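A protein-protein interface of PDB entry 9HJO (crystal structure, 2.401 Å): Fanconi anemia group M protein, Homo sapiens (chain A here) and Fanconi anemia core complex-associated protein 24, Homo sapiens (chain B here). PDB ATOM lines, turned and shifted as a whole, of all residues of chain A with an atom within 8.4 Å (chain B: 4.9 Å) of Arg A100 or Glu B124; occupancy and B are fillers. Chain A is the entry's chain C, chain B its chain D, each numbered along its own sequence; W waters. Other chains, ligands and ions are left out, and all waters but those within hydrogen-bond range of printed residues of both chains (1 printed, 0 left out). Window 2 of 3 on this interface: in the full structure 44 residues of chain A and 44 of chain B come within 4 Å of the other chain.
The guanidinium group of Arg A100 is in hydrogen-bond range of the backbone carbonyl oxygen of Pro B118, 3.0 Å away.
The side-chain carboxylate (OD1) of Asp A105 is in salt-bridge range of the guanidinium group (NE) of Arg A100 (2.7 Å). The side-chain hydroxyl of Thr A109 sits at hydrogen-bond distance from the backbone carbonyl oxygen of Asp A105 (3.2 Å). N of Ala B120 sits at hydrogen-bond distance from OE1 of Glu B124.
Val B119 touches Arg A100. Glu B124 touches Arg A100 (CD to CD, 3.5 Å). Arg A100 touches Leu B128 (NH2 to CD1, 3.6 Å). Cys B127 touches Asp A105. Leu B128 touches Asp A105 (N to OD2, 3.6 Å). Phe A120 touches Pro B118 (CE1 to CD, 3.4 Å).
Arg A100 touches four residues of chain B. Printed residues of chain B within 4 Å of Asp A105: Cys B127 and Leu B128. Ile A112 touches none of the printed residues of chain B. Printed residues of chain B within 4 Å of Phe A120: Pro B118. Of the printed residues of chain A, Pro B118 touches Arg A100 (3.0 Å) and Phe A120 (3.4 Å). Of chain A, only Arg A100 (3.5 Å) comes within 4 Å of Glu B124. Printed residues of chain A within 4 Å of Cys B127: Asp A105 (3.6 Å). Printed residues of chain A within 4 Å of Leu B128: Arg A100 (3.6 Å) and Asp A105 (3.6 Å).
Of the 15 printed residues of chain A, 3 touch a printed residue of chain B. Along chain A the printed residues that touch a printed residue of chain B span positions 100 to 120. Among the printed residues, 7 pairs touch across the chains.
Water W1 lies within hydrogen-bond range of O of Pro B118 (2.8 Å) and NH2 of Arg A100 (2.9 Å).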
ATOM      1  N   GLN A  54     -36.924   5.707   7.670  1.00  0.00           N
ATOM      2  CA  GLN A  54     -35.832   5.789   8.636  1.00  0.00           C
ATOM      3  C   GLN A  54     -35.250   4.407   8.927  1.00  0.00           C
ATOM      4  O   GLN A  54     -34.046   4.223   8.829  1.00  0.00           O
ATOM      5  CB  GLN A  54     -36.305   6.298  10.000  1.00  0.00           C
ATOM      6  CG  GLN A  54     -36.291   7.807  10.172  1.00  0.00           C
ATOM      7  CD  GLN A  54     -37.190   8.236  11.302  1.00  0.00           C
ATOM      8  OE1 GLN A  54     -37.996   7.447  11.811  1.00  0.00           O
ATOM      9  NE2 GLN A  54     -37.079   9.502  11.669  1.00  0.00           N
ATOM     10  N   LEU A  58     -31.524   3.102   8.738  1.00  0.00           N
ATOM     11  CA  LEU A  58     -30.809   2.671   9.942  1.00  0.00           C
ATOM     12  C   LEU A  58     -30.249   1.257   9.779  1.00  0.00           C
ATOM     13  O   LEU A  58     -29.092   1.025  10.128  1.00  0.00           O
ATOM     14  CB  LEU A  58     -31.718   2.766  11.166  1.00  0.00           C
ATOM     15  CG  LEU A  58     -32.109   4.193  11.572  1.00  0.00           C
ATOM     16  CD1 LEU A  58     -33.365   4.283  12.442  1.00  0.00           C
ATOM     17  CD2 LEU A  58     -30.921   4.882  12.240  1.00  0.00           C
ATOM     18  N   PHE A  98     -36.682   5.514  16.591  1.00  0.00           N
ATOM     19  CA  PHE A  98     -35.521   6.066  15.838  1.00  0.00           C
ATOM     20  C   PHE A  98     -34.410   6.386  16.839  1.00  0.00           C
ATOM     21  O   PHE A  98     -34.537   7.322  17.632  1.00  0.00           O
ATOM     22  CB  PHE A  98     -35.964   7.265  14.984  1.00  0.00           C
ATOM     23  CG  PHE A  98     -34.863   8.104  14.336  1.00  0.00           C
ATOM     24  CD1 PHE A  98     -33.670   7.534  13.882  1.00  0.00           C
ATOM     25  CD2 PHE A  98     -35.024   9.485  14.184  1.00  0.00           C
ATOM     26  CE1 PHE A  98     -32.670   8.322  13.320  1.00  0.00           C
ATOM     27  CE2 PHE A  98     -34.026  10.269  13.608  1.00  0.00           C
ATOM     28  CZ  PHE A  98     -32.853   9.687  13.176  1.00  0.00           C
ATOM     29  N   ARG A  99     -33.363   5.547  16.821  1.00  0.00           N
ATOM     30  CA  ARG A  99     -32.041   5.880  17.336  1.00  0.00           C
ATOM     31  C   ARG A  99     -31.054   5.835  16.168  1.00  0.00           C
ATOM     32  O   ARG A  99     -31.069   4.866  15.400  1.00  0.00           O
ATOM     33  CB  ARG A  99     -31.581   4.901  18.425  1.00  0.00           C
ATOM     34  CG  ARG A  99     -32.596   4.556  19.512  1.00  0.00           C
ATOM     35  CD  ARG A  99     -31.974   3.804  20.699  1.00  0.00           C
ATOM     36  NE  ARG A  99     -32.907   2.910  21.399  1.00  0.00           N
ATOM     37  CZ  ARG A  99     -32.566   1.915  22.230  1.00  0.00           C
ATOM     38  NH1 ARG A  99     -31.298   1.685  22.529  1.00  0.00           N
ATOM     39  NH2 ARG A  99     -33.497   1.146  22.773  1.00  0.00           N
ATOM     40  N   ARG A 100     -30.203   6.873  16.051  1.00  0.00           N
ATOM     41  CA  ARG A 100     -29.232   6.984  14.971  1.00  0.00           C
ATOM     42  C   ARG A 100     -28.040   6.083  15.273  1.00  0.00           C
ATOM     43  O   ARG A 100     -27.676   5.899  16.419  1.00  0.00           O
ATOM     44  CB  ARG A 100     -28.570   8.352  14.752  1.00  0.00           C
ATOM     45  CG  ARG A 100     -29.462   9.582  14.698  1.00  0.00           C
ATOM     46  CD  ARG A 100     -28.612  10.822  14.482  1.00  0.00           C
ATOM     47  NE  ARG A 100     -28.190  10.995  13.088  1.00  0.00           N
ATOM     48  CZ  ARG A 100     -28.597  11.957  12.260  1.00  0.00           C
ATOM     49  NH1 ARG A 100     -29.561  12.787  12.601  1.00  0.00           N
ATOM     50  NH2 ARG A 100     -28.029  12.109  11.079  1.00  0.00           N
ATOM     51  N   THR A 101     -27.395   5.627  14.204  1.00  0.00           N
ATOM     52  CA  THR A 101     -26.210   4.794  14.233  1.00  0.00           C
ATOM     53  C   THR A 101     -25.131   5.511  13.427  1.00  0.00           C
ATOM     54  O   THR A 101     -25.446   6.434  12.679  1.00  0.00           O
ATOM     55  CB  THR A 101     -26.566   3.429  13.636  1.00  0.00           C
ATOM     56  OG1 THR A 101     -27.187   3.607  12.367  1.00  0.00           O
ATOM     57  CG2 THR A 101     -27.553   2.655  14.493  1.00  0.00           C
ATOM     58  N   LYS A 102     -23.869   5.084  13.586  1.00  0.00           N
ATOM     59  CA  LYS A 102     -22.760   5.586  12.780  1.00  0.00           C
ATOM     60  C   LYS A 102     -23.024   5.291  11.303  1.00  0.00           C
ATOM     61  O   LYS A 102     -22.879   6.181  10.471  1.00  0.00           O
ATOM     62  CB  LYS A 102     -21.412   5.050  13.291  1.00  0.00           C
ATOM     63  CG  LYS A 102     -20.244   4.973  12.302  1.00  0.00           C
ATOM     64  CD  LYS A 102     -18.874   4.937  12.974  1.00  0.00           C
ATOM     65  CE  LYS A 102     -17.766   4.607  12.009  1.00  0.00           C
ATOM     66  NZ  LYS A 102     -16.451   4.708  12.649  1.00  0.00           N
ATOM     67  N   SER A 103     -23.445   4.052  11.007  1.00  0.00           N
ATOM     68  CA  SER A 103     -23.766   3.570   9.666  1.00  0.00           C
ATOM     69  C   SER A 103     -24.803   4.443   8.956  1.00  0.00           C
ATOM     70  O   SER A 103     -24.731   4.600   7.739  1.00  0.00           O
ATOM     71  CB  SER A 103     -24.260   2.138   9.748  1.00  0.00           C
ATOM     72  OG  SER A 103     -24.550   1.594   8.472  1.00  0.00           O
ATOM     73  N   TYR A 104     -25.776   4.963   9.720  1.00  0.00           N
ATOM     74  CA  TYR A 104     -26.789   5.857   9.201  1.00  0.00           C
ATOM     75  C   TYR A 104     -26.159   7.196   8.848  1.00  0.00           C
ATOM     76  O   TYR A 104     -26.320   7.650   7.718  1.00  0.00           O
ATOM     77  CB  TYR A 104     -27.919   6.074  10.198  1.00  0.00           C
ATOM     78  CG  TYR A 104     -28.982   7.074   9.763  1.00  0.00           C
ATOM     79  CD1 TYR A 104     -30.038   6.698   8.931  1.00  0.00           C
ATOM     80  CD2 TYR A 104     -28.946   8.388  10.212  1.00  0.00           C
ATOM     81  CE1 TYR A 104     -31.028   7.600   8.575  1.00  0.00           C
ATOM     82  CE2 TYR A 104     -29.919   9.302   9.847  1.00  0.00           C
ATOM     83  CZ  TYR A 104     -30.956   8.911   9.016  1.00  0.00           C
ATOM     84  OH  TYR A 104     -31.937   9.796   8.675  1.00  0.00           O
ATOM     85  N   ASP A 105     -25.451   7.813   9.803  1.00  0.00           N
ATOM     86  CA  ASP A 105     -24.732   9.050   9.552  1.00  0.00           C
ATOM     87  C   ASP A 105     -23.742   8.908   8.406  1.00  0.00           C
ATOM     88  O   ASP A 105     -23.623   9.822   7.604  1.00  0.00           O
ATOM     89  CB  ASP A 105     -23.981   9.514  10.780  1.00  0.00           C
ATOM     90  CG  ASP A 105     -24.867  10.061  11.879  1.00  0.00           C
ATOM     91  OD1 ASP A 105     -26.064  10.242  11.590  1.00  0.00           O
ATOM     92  OD2 ASP A 105     -24.347  10.299  12.996  1.00  0.00           O
ATOM     93  N   SER A 106     -23.046   7.770   8.360  1.00  0.00           N
ATOM     94  CA  SER A 106     -22.100   7.417   7.313  1.00  0.00           C
ATOM     95  C   SER A 106     -22.753   7.401   5.926  1.00  0.00           C
ATOM     96  O   SER A 106     -22.142   7.811   4.939  1.00  0.00           O
ATOM     97  CB  SER A 106     -21.486   6.083   7.680  1.00  0.00           C
ATOM     98  OG  SER A 106     -20.619   5.581   6.682  1.00  0.00           O
ATOM     99  N   LEU A 108     -25.615   9.031   5.023  1.00  0.00           N
ATOM    100  CA  LEU A 108     -25.970  10.416   4.754  1.00  0.00           C
ATOM    101  C   LEU A 108     -24.766  11.212   4.258  1.00  0.00           C
ATOM    102  O   LEU A 108     -24.890  11.889   3.244  1.00  0.00           O
ATOM    103  CB  LEU A 108     -26.593  11.098   5.965  1.00  0.00           C
ATOM    104  CG  LEU A 108     -27.951  10.563   6.416  1.00  0.00           C
ATOM    105  CD1 LEU A 108     -28.406  11.330   7.635  1.00  0.00           C
ATOM    106  CD2 LEU A 108     -29.001  10.654   5.327  1.00  0.00           C
ATOM    107  N   THR A 109     -23.617  11.099   4.938  1.00  0.00           N
ATOM    108  CA  THR A 109     -22.420  11.827   4.538  1.00  0.00           C
ATOM    109  C   THR A 109     -21.939  11.314   3.191  1.00  0.00           C
ATOM    110  O   THR A 109     -21.538  12.140   2.384  1.00  0.00           O
ATOM    111  CB  THR A 109     -21.290  11.798   5.571  1.00  0.00           C
ATOM    112  OG1 THR A 109     -21.008  10.437   5.872  1.00  0.00           O
ATOM    113  CG2 THR A 109     -21.649  12.568   6.826  1.00  0.00           C
ATOM    114  N   ILE A 112     -24.183  12.946   0.554  1.00  0.00           N
ATOM    115  CA  ILE A 112     -23.907  14.370   0.441  1.00  0.00           C
ATOM    116  C   ILE A 112     -22.662  14.590  -0.415  1.00  0.00           C
ATOM    117  O   ILE A 112     -22.680  15.464  -1.285  1.00  0.00           O
ATOM    118  CB  ILE A 112     -23.785  15.026   1.835  1.00  0.00           C
ATOM    119  CG1 ILE A 112     -25.134  15.016   2.542  1.00  0.00           C
ATOM    120  CG2 ILE A 112     -23.221  16.451   1.771  1.00  0.00           C
ATOM    121  CD1 ILE A 112     -25.051  15.122   4.051  1.00  0.00           C
ATOM    122  N   PHE A 120     -36.255  15.065   4.079  1.00  0.00           N
ATOM    123  CA  PHE A 120     -36.790  14.380   5.237  1.00  0.00           C
ATOM    124  C   PHE A 120     -38.287  14.672   5.271  1.00  0.00           C
ATOM    125  O   PHE A 120     -38.707  15.809   5.056  1.00  0.00           O
ATOM    126  CB  PHE A 120     -36.034  14.788   6.508  1.00  0.00           C
ATOM    127  CG  PHE A 120     -34.555  14.463   6.387  1.00  0.00           C
ATOM    128  CD1 PHE A 120     -33.682  15.335   5.730  1.00  0.00           C
ATOM    129  CD2 PHE A 120     -34.053  13.257   6.874  1.00  0.00           C
ATOM    130  CE1 PHE A 120     -32.340  15.001   5.554  1.00  0.00           C
ATOM    131  CE2 PHE A 120     -32.707  12.931   6.724  1.00  0.00           C
ATOM    132  CZ  PHE A 120     -31.850  13.800   6.067  1.00  0.00           C
ATOM    133  N   PRO B 118     -31.348  17.080   9.643  1.00  0.00           N
ATOM    134  CA  PRO B 118     -32.028  17.196  10.924  1.00  0.00           C
ATOM    135  C   PRO B 118     -31.306  16.427  12.020  1.00  0.00           C
ATOM    136  O   PRO B 118     -30.659  15.430  11.707  1.00  0.00           O
ATOM    137  CB  PRO B 118     -33.441  16.689  10.662  1.00  0.00           C
ATOM    138  CG  PRO B 118     -33.346  15.863   9.409  1.00  0.00           C
ATOM    139  CD  PRO B 118     -32.069  16.209   8.699  1.00  0.00           C
ATOM    140  N   VAL B 119     -31.411  16.931  13.268  1.00  0.00           N
ATOM    141  CA  VAL B 119     -30.947  16.247  14.474  1.00  0.00           C
ATOM    142  C   VAL B 119     -31.983  16.446  15.585  1.00  0.00           C
ATOM    143  O   VAL B 119     -32.567  17.517  15.710  1.00  0.00           O
ATOM    144  CB  VAL B 119     -29.551  16.702  14.952  1.00  0.00           C
ATOM    145  CG1 VAL B 119     -28.460  16.354  13.943  1.00  0.00           C
ATOM    146  CG2 VAL B 119     -29.511  18.185  15.308  1.00  0.00           C
ATOM    147  N   ALA B 120     -32.196  15.405  16.395  1.00  0.00           N
ATOM    148  CA  ALA B 120     -33.049  15.494  17.572  1.00  0.00           C
ATOM    149  C   ALA B 120     -32.427  16.419  18.622  1.00  0.00           C
ATOM    150  O   ALA B 120     -33.155  17.160  19.279  1.00  0.00           O
ATOM    151  CB  ALA B 120     -33.295  14.117  18.142  1.00  0.00           C
ATOM    152  N   SER B 121     -31.092  16.369  18.756  1.00  0.00           N
ATOM    153  CA  SER B 121     -30.370  17.054  19.814  1.00  0.00           C
ATOM    154  C   SER B 121     -28.931  17.360  19.400  1.00  0.00           C
ATOM    155  O   SER B 121     -28.456  16.846  18.388  1.00  0.00           O
ATOM    156  CB  SER B 121     -30.380  16.189  21.029  1.00  0.00           C
ATOM    157  OG  SER B 121     -29.769  14.935  20.733  1.00  0.00           O
ATOM    158  N   GLN B 122     -28.231  18.143  20.234  1.00  0.00           N
ATOM    159  CA  GLN B 122     -26.811  18.422  20.073  1.00  0.00           C
ATOM    160  C   GLN B 122     -25.959  17.159  20.161  1.00  0.00           C
ATOM    161  O   GLN B 122     -24.925  17.084  19.497  1.00  0.00           O
ATOM    162  CB  GLN B 122     -26.266  19.353  21.149  1.00  0.00           C
ATOM    163  CG  GLN B 122     -26.784  20.779  21.029  1.00  0.00           C
ATOM    164  CD  GLN B 122     -26.025  21.792  21.856  1.00  0.00           C
ATOM    165  OE1 GLN B 122     -24.911  21.559  22.348  1.00  0.00           O
ATOM    166  NE2 GLN B 122     -26.640  22.955  21.981  1.00  0.00           N
ATOM    167  N   MET B 123     -26.378  16.204  21.002  1.00  0.00           N
ATOM    168  CA  MET B 123     -25.707  14.918  21.133  1.00  0.00           C
ATOM    169  C   MET B 123     -25.562  14.253  19.763  1.00  0.00           C
ATOM    170  O   MET B 123     -24.473  13.790  19.427  1.00  0.00           O
ATOM    171  CB  MET B 123     -26.485  14.000  22.083  1.00  0.00           C
ATOM    172  CG  MET B 123     -25.862  12.634  22.319  1.00  0.00           C
ATOM    173  SD  MET B 123     -24.239  12.694  23.106  1.00  0.00           S
ATOM    174  CE  MET B 123     -24.185  11.017  23.763  1.00  0.00           C
ATOM    175  N   GLU B 124     -26.662  14.227  18.989  1.00  0.00           N
ATOM    176  CA  GLU B 124     -26.675  13.654  17.647  1.00  0.00           C
ATOM    177  C   GLU B 124     -25.805  14.469  16.688  1.00  0.00           C
ATOM    178  O   GLU B 124     -25.029  13.891  15.935  1.00  0.00           O
ATOM    179  CB  GLU B 124     -28.095  13.513  17.104  1.00  0.00           C
ATOM    180  CG  GLU B 124     -28.910  12.445  17.828  1.00  0.00           C
ATOM    181  CD  GLU B 124     -30.298  12.207  17.273  1.00  0.00           C
ATOM    182  OE1 GLU B 124     -30.809  13.016  16.455  1.00  0.00           O
ATOM    183  OE2 GLU B 124     -30.831  11.139  17.640  1.00  0.00           O
ATOM    184  N   ALA B 125     -25.897  15.801  16.757  1.00  0.00           N
ATOM    185  CA  ALA B 125     -25.074  16.671  15.936  1.00  0.00           C
ATOM    186  C   ALA B 125     -23.575  16.468  16.174  1.00  0.00           C
ATOM    187  O   ALA B 125     -22.785  16.711  15.265  1.00  0.00           O
ATOM    188  CB  ALA B 125     -25.474  18.105  16.158  1.00  0.00           C
ATOM    189  N   SER B 126     -23.180  16.043  17.384  1.00  0.00           N
ATOM    190  CA  SER B 126     -21.799  15.668  17.654  1.00  0.00           C
ATOM    191  C   SER B 126     -21.377  14.537  16.717  1.00  0.00           C
ATOM    192  O   SER B 126     -20.461  14.702  15.914  1.00  0.00           O
ATOM    193  CB  SER B 126     -21.592  15.273  19.109  1.00  0.00           C
ATOM    194  OG  SER B 126     -22.462  16.000  19.963  1.00  0.00           O
ATOM    195  N   CYS B 127     -22.097  13.410  16.800  1.00  0.00           N
ATOM    196  CA  CYS B 127     -21.735  12.188  16.096  1.00  0.00           C
ATOM    197  C   CYS B 127     -21.877  12.359  14.575  1.00  0.00           C
ATOM    198  O   CYS B 127     -21.170  11.687  13.820  1.00  0.00           O
ATOM    199  CB  CYS B 127     -22.511  10.991  16.658  1.00  0.00           C
ATOM    200  SG  CYS B 127     -21.861  10.331  18.219  1.00  0.00           S
ATOM    201  N   LEU B 128     -22.762  13.274  14.134  1.00  0.00           N
ATOM    202  CA  LEU B 128     -22.953  13.608  12.728  1.00  0.00           C
ATOM    203  C   LEU B 128     -21.792  14.433  12.176  1.00  0.00           C
ATOM    204  O   LEU B 128     -21.378  14.212  11.038  1.00  0.00           O
ATOM    205  CB  LEU B 128     -24.260  14.381  12.551  1.00  0.00           C
ATOM    206  CG  LEU B 128     -24.639  14.752  11.116  1.00  0.00           C
ATOM    207  CD1 LEU B 128     -24.820  13.514  10.281  1.00  0.00           C
ATOM    208  CD2 LEU B 128     -25.887  15.601  11.108  1.00  0.00           C
HETATM  209  O   HOH W   1     -29.957  13.661   9.596  1.00  0.00           O
